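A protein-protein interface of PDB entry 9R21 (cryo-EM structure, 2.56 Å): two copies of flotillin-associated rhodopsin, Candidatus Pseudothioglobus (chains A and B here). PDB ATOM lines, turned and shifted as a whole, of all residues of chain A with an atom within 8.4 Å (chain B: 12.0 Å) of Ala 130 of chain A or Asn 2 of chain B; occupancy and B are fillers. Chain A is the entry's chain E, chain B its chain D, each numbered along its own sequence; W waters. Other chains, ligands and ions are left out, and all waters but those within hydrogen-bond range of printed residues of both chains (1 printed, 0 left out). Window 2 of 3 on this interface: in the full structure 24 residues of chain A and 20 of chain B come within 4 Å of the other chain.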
ATOM      1  N   VAL A  74      10.015   1.071 -22.442  1.00  0.00           N
ATOM      2  CA  VAL A  74       8.938   0.594 -23.298  1.00  0.00           C
ATOM      3  C   VAL A  74       9.225  -0.836 -23.759  1.00  0.00           C
ATOM      4  O   VAL A  74       8.313  -1.545 -24.135  1.00  0.00           O
ATOM      5  CB  VAL A  74       8.793   1.511 -24.519  1.00  0.00           C
ATOM      6  CG1 VAL A  74       9.828   1.172 -25.575  1.00  0.00           C
ATOM      7  CG2 VAL A  74       7.422   1.418 -25.164  1.00  0.00           C
ATOM      8  N   GLY A 119      -2.919  -1.447 -22.466  1.00  0.00           N
ATOM      9  CA  GLY A 119      -3.330  -0.085 -22.190  1.00  0.00           C
ATOM     10  C   GLY A 119      -2.132   0.760 -21.776  1.00  0.00           C
ATOM     11  O   GLY A 119      -1.921   1.850 -22.278  1.00  0.00           O
ATOM     12  N   GLU A 120      -1.321   0.218 -20.884  1.00  0.00           N
ATOM     13  CA  GLU A 120      -0.142   0.908 -20.398  1.00  0.00           C
ATOM     14  C   GLU A 120       0.885   1.056 -21.527  1.00  0.00           C
ATOM     15  O   GLU A 120       1.545   2.084 -21.604  1.00  0.00           O
ATOM     16  CB  GLU A 120       0.270   0.032 -19.223  1.00  0.00           C
ATOM     17  CG  GLU A 120       1.274   0.623 -18.248  1.00  0.00           C
ATOM     18  CD  GLU A 120       1.864  -0.381 -17.242  1.00  0.00           C
ATOM     19  OE1 GLU A 120       3.109  -0.628 -17.246  1.00  0.00           O
ATOM     20  OE2 GLU A 120       1.059  -0.920 -16.434  1.00  0.00           O
ATOM     21  N   PHE A 121       0.933   0.103 -22.471  1.00  0.00           N
ATOM     22  CA  PHE A 121       1.802   0.188 -23.635  1.00  0.00           C
ATOM     23  C   PHE A 121       1.347   1.264 -24.611  1.00  0.00           C
ATOM     24  O   PHE A 121       2.171   1.907 -25.238  1.00  0.00           O
ATOM     25  CB  PHE A 121       1.939  -1.112 -24.409  1.00  0.00           C
ATOM     26  CG  PHE A 121       2.606  -0.926 -25.764  1.00  0.00           C
ATOM     27  CD1 PHE A 121       1.840  -0.784 -26.927  1.00  0.00           C
ATOM     28  CD2 PHE A 121       3.987  -0.927 -25.887  1.00  0.00           C
ATOM     29  CE1 PHE A 121       2.442  -0.613 -28.155  1.00  0.00           C
ATOM     30  CE2 PHE A 121       4.580  -0.727 -27.120  1.00  0.00           C
ATOM     31  CZ  PHE A 121       3.809  -0.548 -28.246  1.00  0.00           C
ATOM     32  N   LEU A 122       0.060   1.500 -24.748  1.00  0.00           N
ATOM     33  CA  LEU A 122      -0.365   2.570 -25.627  1.00  0.00           C
ATOM     34  C   LEU A 122       0.032   3.938 -25.056  1.00  0.00           C
ATOM     35  O   LEU A 122       0.668   4.728 -25.748  1.00  0.00           O
ATOM     36  CB  LEU A 122      -1.864   2.405 -25.866  1.00  0.00           C
ATOM     37  CG  LEU A 122      -2.246   1.136 -26.643  1.00  0.00           C
ATOM     38  CD1 LEU A 122      -3.730   0.864 -26.517  1.00  0.00           C
ATOM     39  CD2 LEU A 122      -1.802   1.209 -28.095  1.00  0.00           C
ATOM     40  N   GLY A 123      -0.271   4.219 -23.789  1.00  0.00           N
ATOM     41  CA  GLY A 123       0.202   5.448 -23.174  1.00  0.00           C
ATOM     42  C   GLY A 123       1.735   5.597 -23.182  1.00  0.00           C
ATOM     43  O   GLY A 123       2.260   6.706 -23.232  1.00  0.00           O
ATOM     44  N   ALA A 124       2.464   4.499 -23.071  1.00  0.00           N
ATOM     45  CA  ALA A 124       3.903   4.589 -22.991  1.00  0.00           C
ATOM     46  C   ALA A 124       4.521   4.930 -24.342  1.00  0.00           C
ATOM     47  O   ALA A 124       5.509   5.664 -24.404  1.00  0.00           O
ATOM     48  CB  ALA A 124       4.469   3.272 -22.506  1.00  0.00           C
ATOM     49  N   ALA A 125       3.965   4.352 -25.405  1.00  0.00           N
ATOM     50  CA  ALA A 125       4.483   4.495 -26.751  1.00  0.00           C
ATOM     51  C   ALA A 125       3.825   5.665 -27.489  1.00  0.00           C
ATOM     52  O   ALA A 125       3.946   5.756 -28.695  1.00  0.00           O
ATOM     53  CB  ALA A 125       4.234   3.197 -27.488  1.00  0.00           C
ATOM     54  N   GLY A 126       3.067   6.526 -26.812  1.00  0.00           N
ATOM     55  CA  GLY A 126       2.592   7.732 -27.454  1.00  0.00           C
ATOM     56  C   GLY A 126       1.309   7.563 -28.276  1.00  0.00           C
ATOM     57  O   GLY A 126       0.826   8.545 -28.828  1.00  0.00           O
ATOM     58  N   TYR A 127       0.706   6.377 -28.329  1.00  0.00           N
ATOM     59  CA  TYR A 127      -0.483   6.194 -29.147  1.00  0.00           C
ATOM     60  C   TYR A 127      -1.720   6.772 -28.474  1.00  0.00           C
ATOM     61  O   TYR A 127      -2.649   7.138 -29.174  1.00  0.00           O
ATOM     62  CB  TYR A 127      -0.674   4.734 -29.539  1.00  0.00           C
ATOM     63  CG  TYR A 127       0.555   4.216 -30.289  1.00  0.00           C
ATOM     64  CD1 TYR A 127       1.148   4.945 -31.311  1.00  0.00           C
ATOM     65  CD2 TYR A 127       1.143   3.009 -29.961  1.00  0.00           C
ATOM     66  CE1 TYR A 127       2.267   4.493 -31.984  1.00  0.00           C
ATOM     67  CE2 TYR A 127       2.266   2.546 -30.619  1.00  0.00           C
ATOM     68  CZ  TYR A 127       2.838   3.290 -31.632  1.00  0.00           C
ATOM     69  OH  TYR A 127       3.954   2.818 -32.266  1.00  0.00           O
ATOM     70  N   MET A 128      -1.770   6.854 -27.144  1.00  0.00           N
ATOM     71  CA  MET A 128      -2.880   7.537 -26.493  1.00  0.00           C
ATOM     72  C   MET A 128      -2.343   8.267 -25.277  1.00  0.00           C
ATOM     73  O   MET A 128      -1.161   8.145 -24.981  1.00  0.00           O
ATOM     74  CB  MET A 128      -4.031   6.589 -26.140  1.00  0.00           C
ATOM     75  CG  MET A 128      -3.707   5.472 -25.177  1.00  0.00           C
ATOM     76  SD  MET A 128      -5.256   4.614 -24.810  1.00  0.00           S
ATOM     77  CE  MET A 128      -4.547   3.198 -23.952  1.00  0.00           C
ATOM     78  N   SER A 129      -3.179   9.073 -24.625  1.00  0.00           N
ATOM     79  CA  SER A 129      -2.679   9.908 -23.554  1.00  0.00           C
ATOM     80  C   SER A 129      -2.079   8.994 -22.506  1.00  0.00           C
ATOM     81  O   SER A 129      -2.655   7.939 -22.250  1.00  0.00           O
ATOM     82  CB  SER A 129      -3.732  10.761 -22.947  1.00  0.00           C
ATOM     83  OG  SER A 129      -4.807   9.966 -22.475  1.00  0.00           O
ATOM     84  N   ALA A 130      -0.944   9.411 -21.922  1.00  0.00           N
ATOM     85  CA  ALA A 130      -0.354   8.699 -20.812  1.00  0.00           C
ATOM     86  C   ALA A 130      -1.350   8.613 -19.661  1.00  0.00           C
ATOM     87  O   ALA A 130      -1.445   7.585 -18.987  1.00  0.00           O
ATOM     88  CB  ALA A 130       0.864   9.411 -20.375  1.00  0.00           C
ATOM     89  N   THR A 131      -2.151   9.656 -19.462  1.00  0.00           N
ATOM     90  CA  THR A 131      -3.156   9.527 -18.436  1.00  0.00           C
ATOM     91  C   THR A 131      -4.034   8.333 -18.698  1.00  0.00           C
ATOM     92  O   THR A 131      -4.435   7.671 -17.753  1.00  0.00           O
ATOM     93  CB  THR A 131      -4.061  10.729 -18.316  1.00  0.00           C
ATOM     94  OG1 THR A 131      -3.129  11.800 -18.383  1.00  0.00           O
ATOM     95  CG2 THR A 131      -4.810  10.673 -17.007  1.00  0.00           C
ATOM     96  N   LEU A 132      -4.412   8.123 -19.951  1.00  0.00           N
ATOM     97  CA  LEU A 132      -5.492   7.195 -20.215  1.00  0.00           C
ATOM     98  C   LEU A 132      -4.923   5.787 -20.136  1.00  0.00           C
ATOM     99  O   LEU A 132      -5.551   4.882 -19.594  1.00  0.00           O
ATOM    100  CB  LEU A 132      -6.161   7.513 -21.542  1.00  0.00           C
ATOM    101  CG  LEU A 132      -7.214   6.520 -22.016  1.00  0.00           C
ATOM    102  CD1 LEU A 132      -8.397   6.439 -21.085  1.00  0.00           C
ATOM    103  CD2 LEU A 132      -7.627   6.963 -23.393  1.00  0.00           C
ATOM    104  N   GLY A 133      -3.691   5.632 -20.575  1.00  0.00           N
ATOM    105  CA  GLY A 133      -3.066   4.334 -20.492  1.00  0.00           C
ATOM    106  C   GLY A 133      -2.829   3.899 -19.051  1.00  0.00           C
ATOM    107  O   GLY A 133      -2.668   2.708 -18.812  1.00  0.00           O
ATOM    108  N   PHE A 134      -2.696   4.855 -18.132  1.00  0.00           N
ATOM    109  CA  PHE A 134      -2.578   4.559 -16.712  1.00  0.00           C
ATOM    110  C   PHE A 134      -3.907   4.012 -16.197  1.00  0.00           C
ATOM    111  O   PHE A 134      -4.004   2.882 -15.750  1.00  0.00           O
ATOM    112  CB  PHE A 134      -2.224   5.841 -15.958  1.00  0.00           C
ATOM    113  CG  PHE A 134      -2.117   5.636 -14.461  1.00  0.00           C
ATOM    114  CD1 PHE A 134      -2.981   6.291 -13.585  1.00  0.00           C
ATOM    115  CD2 PHE A 134      -1.153   4.772 -13.930  1.00  0.00           C
ATOM    116  CE1 PHE A 134      -2.853   6.109 -12.211  1.00  0.00           C
ATOM    117  CE2 PHE A 134      -1.049   4.580 -12.553  1.00  0.00           C
ATOM    118  CZ  PHE A 134      -1.895   5.248 -11.708  1.00  0.00           C
ATOM    119  N   ILE A 135      -4.945   4.827 -16.323  1.00  0.00           N
ATOM    120  CA  ILE A 135      -6.282   4.430 -15.972  1.00  0.00           C
ATOM    121  C   ILE A 135      -6.634   3.053 -16.516  1.00  0.00           C
ATOM    122  O   ILE A 135      -7.311   2.294 -15.828  1.00  0.00           O
ATOM    123  CB  ILE A 135      -7.282   5.447 -16.496  1.00  0.00           C
ATOM    124  CG1 ILE A 135      -7.168   6.717 -15.781  1.00  0.00           C
ATOM    125  CG2 ILE A 135      -8.690   4.884 -16.356  1.00  0.00           C
ATOM    126  CD1 ILE A 135      -7.930   7.819 -16.463  1.00  0.00           C
ATOM    127  N   ILE A 136      -6.328   2.783 -17.782  1.00  0.00           N
ATOM    128  CA  ILE A 136      -6.717   1.507 -18.353  1.00  0.00           C
ATOM    129  C   ILE A 136      -5.858   0.423 -17.716  1.00  0.00           C
ATOM    130  O   ILE A 136      -6.371  -0.608 -17.318  1.00  0.00           O
ATOM    131  CB  ILE A 136      -6.599   1.484 -19.884  1.00  0.00           C
ATOM    132  CG1 ILE A 136      -7.669   2.296 -20.543  1.00  0.00           C
ATOM    133  CG2 ILE A 136      -6.570   0.061 -20.432  1.00  0.00           C
ATOM    134  CD1 ILE A 136      -7.308   2.641 -21.970  1.00  0.00           C
ATOM    135  N   GLY A 137      -4.570   0.645 -17.589  1.00  0.00           N
ATOM    136  CA  GLY A 137      -3.712  -0.350 -16.969  1.00  0.00           C
ATOM    137  C   GLY A 137      -4.126  -0.669 -15.530  1.00  0.00           C
ATOM    138  O   GLY A 137      -4.029  -1.811 -15.100  1.00  0.00           O
ATOM    139  N   TYR A 187       4.931   3.221 -14.020  1.00  0.00           N
ATOM    140  CA  TYR A 187       4.234   3.941 -15.061  1.00  0.00           C
ATOM    141  C   TYR A 187       3.864   5.332 -14.567  1.00  0.00           C
ATOM    142  O   TYR A 187       4.152   6.314 -15.204  1.00  0.00           O
ATOM    143  CB  TYR A 187       2.975   3.152 -15.464  1.00  0.00           C
ATOM    144  CG  TYR A 187       2.250   3.793 -16.640  1.00  0.00           C
ATOM    145  CD1 TYR A 187       1.412   4.881 -16.435  1.00  0.00           C
ATOM    146  CD2 TYR A 187       2.515   3.428 -17.957  1.00  0.00           C
ATOM    147  CE1 TYR A 187       0.817   5.541 -17.495  1.00  0.00           C
ATOM    148  CE2 TYR A 187       1.884   4.047 -19.026  1.00  0.00           C
ATOM    149  CZ  TYR A 187       1.030   5.105 -18.788  1.00  0.00           C
ATOM    150  OH  TYR A 187       0.383   5.803 -19.755  1.00  0.00           O
ATOM    151  N   PHE A 188       3.186   5.424 -13.449  1.00  0.00           N
ATOM    152  CA  PHE A 188       2.772   6.715 -12.983  1.00  0.00           C
ATOM    153  C   PHE A 188       3.950   7.678 -12.931  1.00  0.00           C
ATOM    154  O   PHE A 188       3.846   8.808 -13.395  1.00  0.00           O
ATOM    155  CB  PHE A 188       2.170   6.627 -11.593  1.00  0.00           C
ATOM    156  CG  PHE A 188       1.645   7.991 -11.221  1.00  0.00           C
ATOM    157  CD1 PHE A 188       2.497   8.947 -10.707  1.00  0.00           C
ATOM    158  CD2 PHE A 188       0.320   8.328 -11.468  1.00  0.00           C
ATOM    159  CE1 PHE A 188       2.011  10.203 -10.389  1.00  0.00           C
ATOM    160  CE2 PHE A 188      -0.151   9.588 -11.159  1.00  0.00           C
ATOM    161  CZ  PHE A 188       0.698  10.520 -10.612  1.00  0.00           C
ATOM    162  N   ILE A 189       5.086   7.240 -12.397  1.00  0.00           N
ATOM    163  CA  ILE A 189       6.188   8.159 -12.179  1.00  0.00           C
ATOM    164  C   ILE A 189       6.860   8.434 -13.511  1.00  0.00           C
ATOM    165  O   ILE A 189       7.048   9.588 -13.883  1.00  0.00           O
ATOM    166  CB  ILE A 189       7.191   7.634 -11.145  1.00  0.00           C
ATOM    167  CG1 ILE A 189       6.461   7.082  -9.937  1.00  0.00           C
ATOM    168  CG2 ILE A 189       8.109   8.772 -10.741  1.00  0.00           C
ATOM    169  CD1 ILE A 189       7.354   6.709  -8.784  1.00  0.00           C
ATOM    170  N   ASN A 190       7.222   7.370 -14.215  1.00  0.00           N
ATOM    171  CA  ASN A 190       7.931   7.542 -15.458  1.00  0.00           C
ATOM    172  C   ASN A 190       7.153   8.472 -16.395  1.00  0.00           C
ATOM    173  O   ASN A 190       7.773   9.299 -17.061  1.00  0.00           O
ATOM    174  CB  ASN A 190       8.201   6.217 -16.128  1.00  0.00           C
ATOM    175  CG  ASN A 190       9.154   6.408 -17.265  1.00  0.00           C
ATOM    176  OD1 ASN A 190       9.880   7.411 -17.283  1.00  0.00           O
ATOM    177  ND2 ASN A 190       9.167   5.469 -18.201  1.00  0.00           N
ATOM    178  N   ASN A 191       5.816   8.382 -16.433  1.00  0.00           N
ATOM    179  CA  ASN A 191       5.044   9.044 -17.480  1.00  0.00           C
ATOM    180  C   ASN A 191       4.227  10.197 -16.905  1.00  0.00           C
ATOM    181  O   ASN A 191       4.333  11.335 -17.340  1.00  0.00           O
ATOM    182  CB  ASN A 191       4.121   8.086 -18.222  1.00  0.00           C
ATOM    183  CG  ASN A 191       4.891   6.906 -18.733  1.00  0.00           C
ATOM    184  OD1 ASN A 191       5.745   7.056 -19.610  1.00  0.00           O
ATOM    185  ND2 ASN A 191       4.636   5.732 -18.191  1.00  0.00           N
ATOM    186  N   LEU A 192       3.384   9.906 -15.941  1.00  0.00           N
ATOM    187  CA  LEU A 192       2.384  10.876 -15.548  1.00  0.00           C
ATOM    188  C   LEU A 192       2.935  11.819 -14.482  1.00  0.00           C
ATOM    189  O   LEU A 192       2.311  12.808 -14.102  1.00  0.00           O
ATOM    190  CB  LEU A 192       1.158  10.107 -15.057  1.00  0.00           C
ATOM    191  CG  LEU A 192       0.081   9.915 -16.101  1.00  0.00           C
ATOM    192  CD1 LEU A 192      -1.048   9.355 -15.288  1.00  0.00           C
ATOM    193  CD2 LEU A 192      -0.213  11.269 -16.726  1.00  0.00           C
ATOM    194  N   GLY A 193       4.098  11.481 -13.966  1.00  0.00           N
ATOM    195  CA  GLY A 193       4.587  12.159 -12.784  1.00  0.00           C
ATOM    196  C   GLY A 193       5.841  12.947 -13.121  1.00  0.00           C
ATOM    197  O   GLY A 193       6.098  13.266 -14.283  1.00  0.00           O
ATOM    198  N   ASN B   2       3.416  10.939 -24.419  1.00  0.00           N
ATOM    199  CA  ASN B   2       4.850  10.649 -24.739  1.00  0.00           C
ATOM    200  C   ASN B   2       5.098  10.939 -26.226  1.00  0.00           C
ATOM    201  O   ASN B   2       4.209  11.450 -26.913  1.00  0.00           O
ATOM    202  CB  ASN B   2       5.215   9.218 -24.344  1.00  0.00           C
ATOM    203  CG  ASN B   2       4.958   8.925 -22.881  1.00  0.00           C
ATOM    204  OD1 ASN B   2       3.803   8.930 -22.434  1.00  0.00           O
ATOM    205  ND2 ASN B   2       6.015   8.663 -22.119  1.00  0.00           N
ATOM    206  N   SER B   3       6.310  10.630 -26.716  1.00  0.00           N
ATOM    207  CA  SER B   3       6.649  10.765 -28.130  1.00  0.00           C
ATOM    208  C   SER B   3       6.484   9.416 -28.820  1.00  0.00           C
ATOM    209  O   SER B   3       7.042   8.420 -28.360  1.00  0.00           O
ATOM    210  CB  SER B   3       8.051  11.291 -28.299  1.00  0.00           C
ATOM    211  OG  SER B   3       8.936  10.684 -27.366  1.00  0.00           O
ATOM    212  N   THR B   4       5.720   9.392 -29.911  1.00  0.00           N
ATOM    213  CA  THR B   4       5.235   8.130 -30.439  1.00  0.00           C
ATOM    214  C   THR B   4       6.438   7.245 -30.735  1.00  0.00           C
ATOM    215  O   THR B   4       7.525   7.737 -31.029  1.00  0.00           O
ATOM    216  CB  THR B   4       4.319   8.361 -31.641  1.00  0.00           C
ATOM    217  OG1 THR B   4       4.144   9.773 -31.691  1.00  0.00           O
ATOM    218  CG2 THR B   4       2.942   7.742 -31.469  1.00  0.00           C
ATOM    219  N   LEU B   5       6.258   5.941 -30.555  1.00  0.00           N
ATOM    220  CA  LEU B   5       7.243   5.007 -31.045  1.00  0.00           C
ATOM    221  C   LEU B   5       7.186   5.052 -32.573  1.00  0.00           C
ATOM    222  O   LEU B   5       6.121   5.271 -33.151  1.00  0.00           O
ATOM    223  CB  LEU B   5       6.947   3.620 -30.491  1.00  0.00           C
ATOM    224  CG  LEU B   5       7.683   3.230 -29.224  1.00  0.00           C
ATOM    225  CD1 LEU B   5       7.467   1.749 -29.086  1.00  0.00           C
ATOM    226  CD2 LEU B   5       9.148   3.556 -29.291  1.00  0.00           C
ATOM    227  N   LEU B   6       8.333   4.862 -33.228  1.00  0.00           N
ATOM    228  CA  LEU B   6       8.384   4.807 -34.680  1.00  0.00           C
ATOM    229  C   LEU B   6       8.127   3.380 -35.147  1.00  0.00           C
ATOM    230  O   LEU B   6       8.447   2.427 -34.441  1.00  0.00           O
ATOM    231  CB  LEU B   6       9.746   5.287 -35.172  1.00  0.00           C
ATOM    232  CG  LEU B   6      10.143   6.704 -34.754  1.00  0.00           C
ATOM    233  CD1 LEU B   6      11.576   6.976 -35.160  1.00  0.00           C
ATOM    234  CD2 LEU B   6       9.180   7.730 -35.332  1.00  0.00           C
ATOM    235  N   ASP B   9      10.739   0.969 -34.616  1.00  0.00           N
ATOM    236  CA  ASP B   9      10.883   0.492 -33.246  1.00  0.00           C
ATOM    237  C   ASP B   9       9.920  -0.661 -33.011  1.00  0.00           C
ATOM    238  O   ASP B   9      10.280  -1.640 -32.362  1.00  0.00           O
ATOM    239  CB  ASP B   9      10.595   1.587 -32.241  1.00  0.00           C
ATOM    240  CG  ASP B   9      11.424   2.855 -32.399  1.00  0.00           C
ATOM    241  OD1 ASP B   9      10.811   3.926 -32.578  1.00  0.00           O
ATOM    242  OD2 ASP B   9      12.676   2.772 -32.302  1.00  0.00           O
ATOM    243  N   ILE B  10       8.727  -0.559 -33.601  1.00  0.00           N
ATOM    244  CA  ILE B  10       7.743  -1.615 -33.496  1.00  0.00           C
ATOM    245  C   ILE B  10       8.173  -2.836 -34.302  1.00  0.00           C
ATOM    246  O   ILE B  10       8.059  -3.951 -33.808  1.00  0.00           O
ATOM    247  CB  ILE B  10       6.365  -1.115 -33.916  1.00  0.00           C
ATOM    248  CG1 ILE B  10       6.010   0.204 -33.242  1.00  0.00           C
ATOM    249  CG2 ILE B  10       5.329  -2.192 -33.625  1.00  0.00           C
ATOM    250  CD1 ILE B  10       5.935   0.095 -31.733  1.00  0.00           C
HETATM  251  O   HOH W   1       1.290   8.653 -24.315  1.00  0.00           O
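Water W1 lies within hydrogen-bond range of O of Gly 123 of chain A (2.4 Å), O of Met 128 of chain A (2.6 Å), N of Asn 2 of chain B (3.1 Å) and N of Ala 130 of chain A (3.4 Å).
Hydrophobic or aromatic side chains of chain B within 4 Å of the printed part of chain A: Leu 5 and Ile 10. Hydrophobic or aromatic side chains of chain A that line the printed part of chain B: Val 74, Ala 125, Tyr 127 and Ala 130. Among the printed residues, 11 pairs touch across the chains. Among the printed residues, no Asp or Glu carboxylate lies within 4 Å of a Lys or Arg side-chain nitrogen of the other chain.
No position is printed for both chains. Of the 11 pairs that touch across the chains among the printed residues, none has its exchanged pair printed and touching as well.
The side-chain hydroxyl (OH) of Tyr 187 of chain A lies within hydrogen-bond range of the backbone carbonyl oxygen (O) of Ala 130 of chain A (2.7 Å). The backbone carbonyl oxygen (O) of Tyr 187 of chain A lies within hydrogen-bond range of the side-chain amide nitrogen (ND2) of Asn 191 of chain A (3.1 Å). N of Tyr 127 of chain A sits at hydrogen-bond distance from O of Leu 122 of chain A, 3.1 Å away.
The backbone carbonyl oxygen (O) of Leu 5 of chain B is in hydrogen-bond range of the side-chain hydroxyl (OH) of Tyr 127 of chain A. The backbone carbonyl oxygen of Ala 125 of chain A lies within hydrogen-bond range of the backbone NH of Leu 5 of chain B (3.0 Å). OD1 of Asn 2 of chain B sits close to O of Gly 123 of chain A (2.8 Å). The side-chain amide nitrogen of Asn 2 of chain B lies within hydrogen-bond range of the side-chain amide oxygen of Asn 191 of chain A, 3.0 Å away.
Among the printed residues, merely in contact across the chains: Val 74 of chain A with Leu 5 of chain B (3.9 Å), Ala 124 of chain A with Asn 2 of chain B (3.6 Å), Ala 125 of chain A with Thr 4 of chain B (3.2 Å), Gly 126 of chain A with Thr 4 of chain B (3.5 Å), Tyr 127 of chain A with Thr 4 of chain B (3.3 Å), Tyr 127 of chain A with Ile 10 of chain B (3.4 Å) and Ala 130 of chain A with Asn 2 of chain B (3.6 Å).
Ala 130 of chain A touches one residue of chain B. Asn 2 of chain B touches just these residues of chain A: Gly 123, Ala 124, Ala 130 and Asn 191. Of chain B, only Asn 2 comes within 4 Å of Gly 123 of chain A. Ala 125 of chain A touches just these residues of chain B: Thr 4 (3.2 Å) and Leu 5 (3.0 Å). Of chain B, only Thr 4 comes within 4 Å of Gly 126 of chain A. No residue of chain B comes within 4 Å of Ser 129 of chain A. No residue of chain B comes within 4 Å of Thr 131 of chain A. No residue of chain B comes within 4 Å of Gly 133 of chain A. No residue of chain B comes within 4 Å of Phe 134 of chain A. Of chain B, only Asn 2 comes within 4 Å of Asn 191 of chain A. No residue of chain B comes within 4 Å of Leu 192 of chain A. No residue of chain A comes within 4 Å of Ser 3 of chain B. Printed residues of chain A within 4 Å of Thr 4 of chain B: Ala 125 (3.2 Å), Gly 126 (3.5 Å) and Tyr 127 (3.3 Å). Of the printed residues of chain B, Tyr 127 of chain A touches Thr 4, Leu 5 and Ile 10. Phe 121 of chain A touches none of the printed residues of chain B. The nearest residue of chain B that does not touch Ala 130 of chain A is Ser 3 of chain B (8.4 Å). The nearest residue of chain A that does not touch Asn 2 of chain B is Gly 126 of chain A (4.1 Å). The nearest printed residue of chain A that does not touch Leu 5 of chain B is Phe 121 of chain A (4.3 Å).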
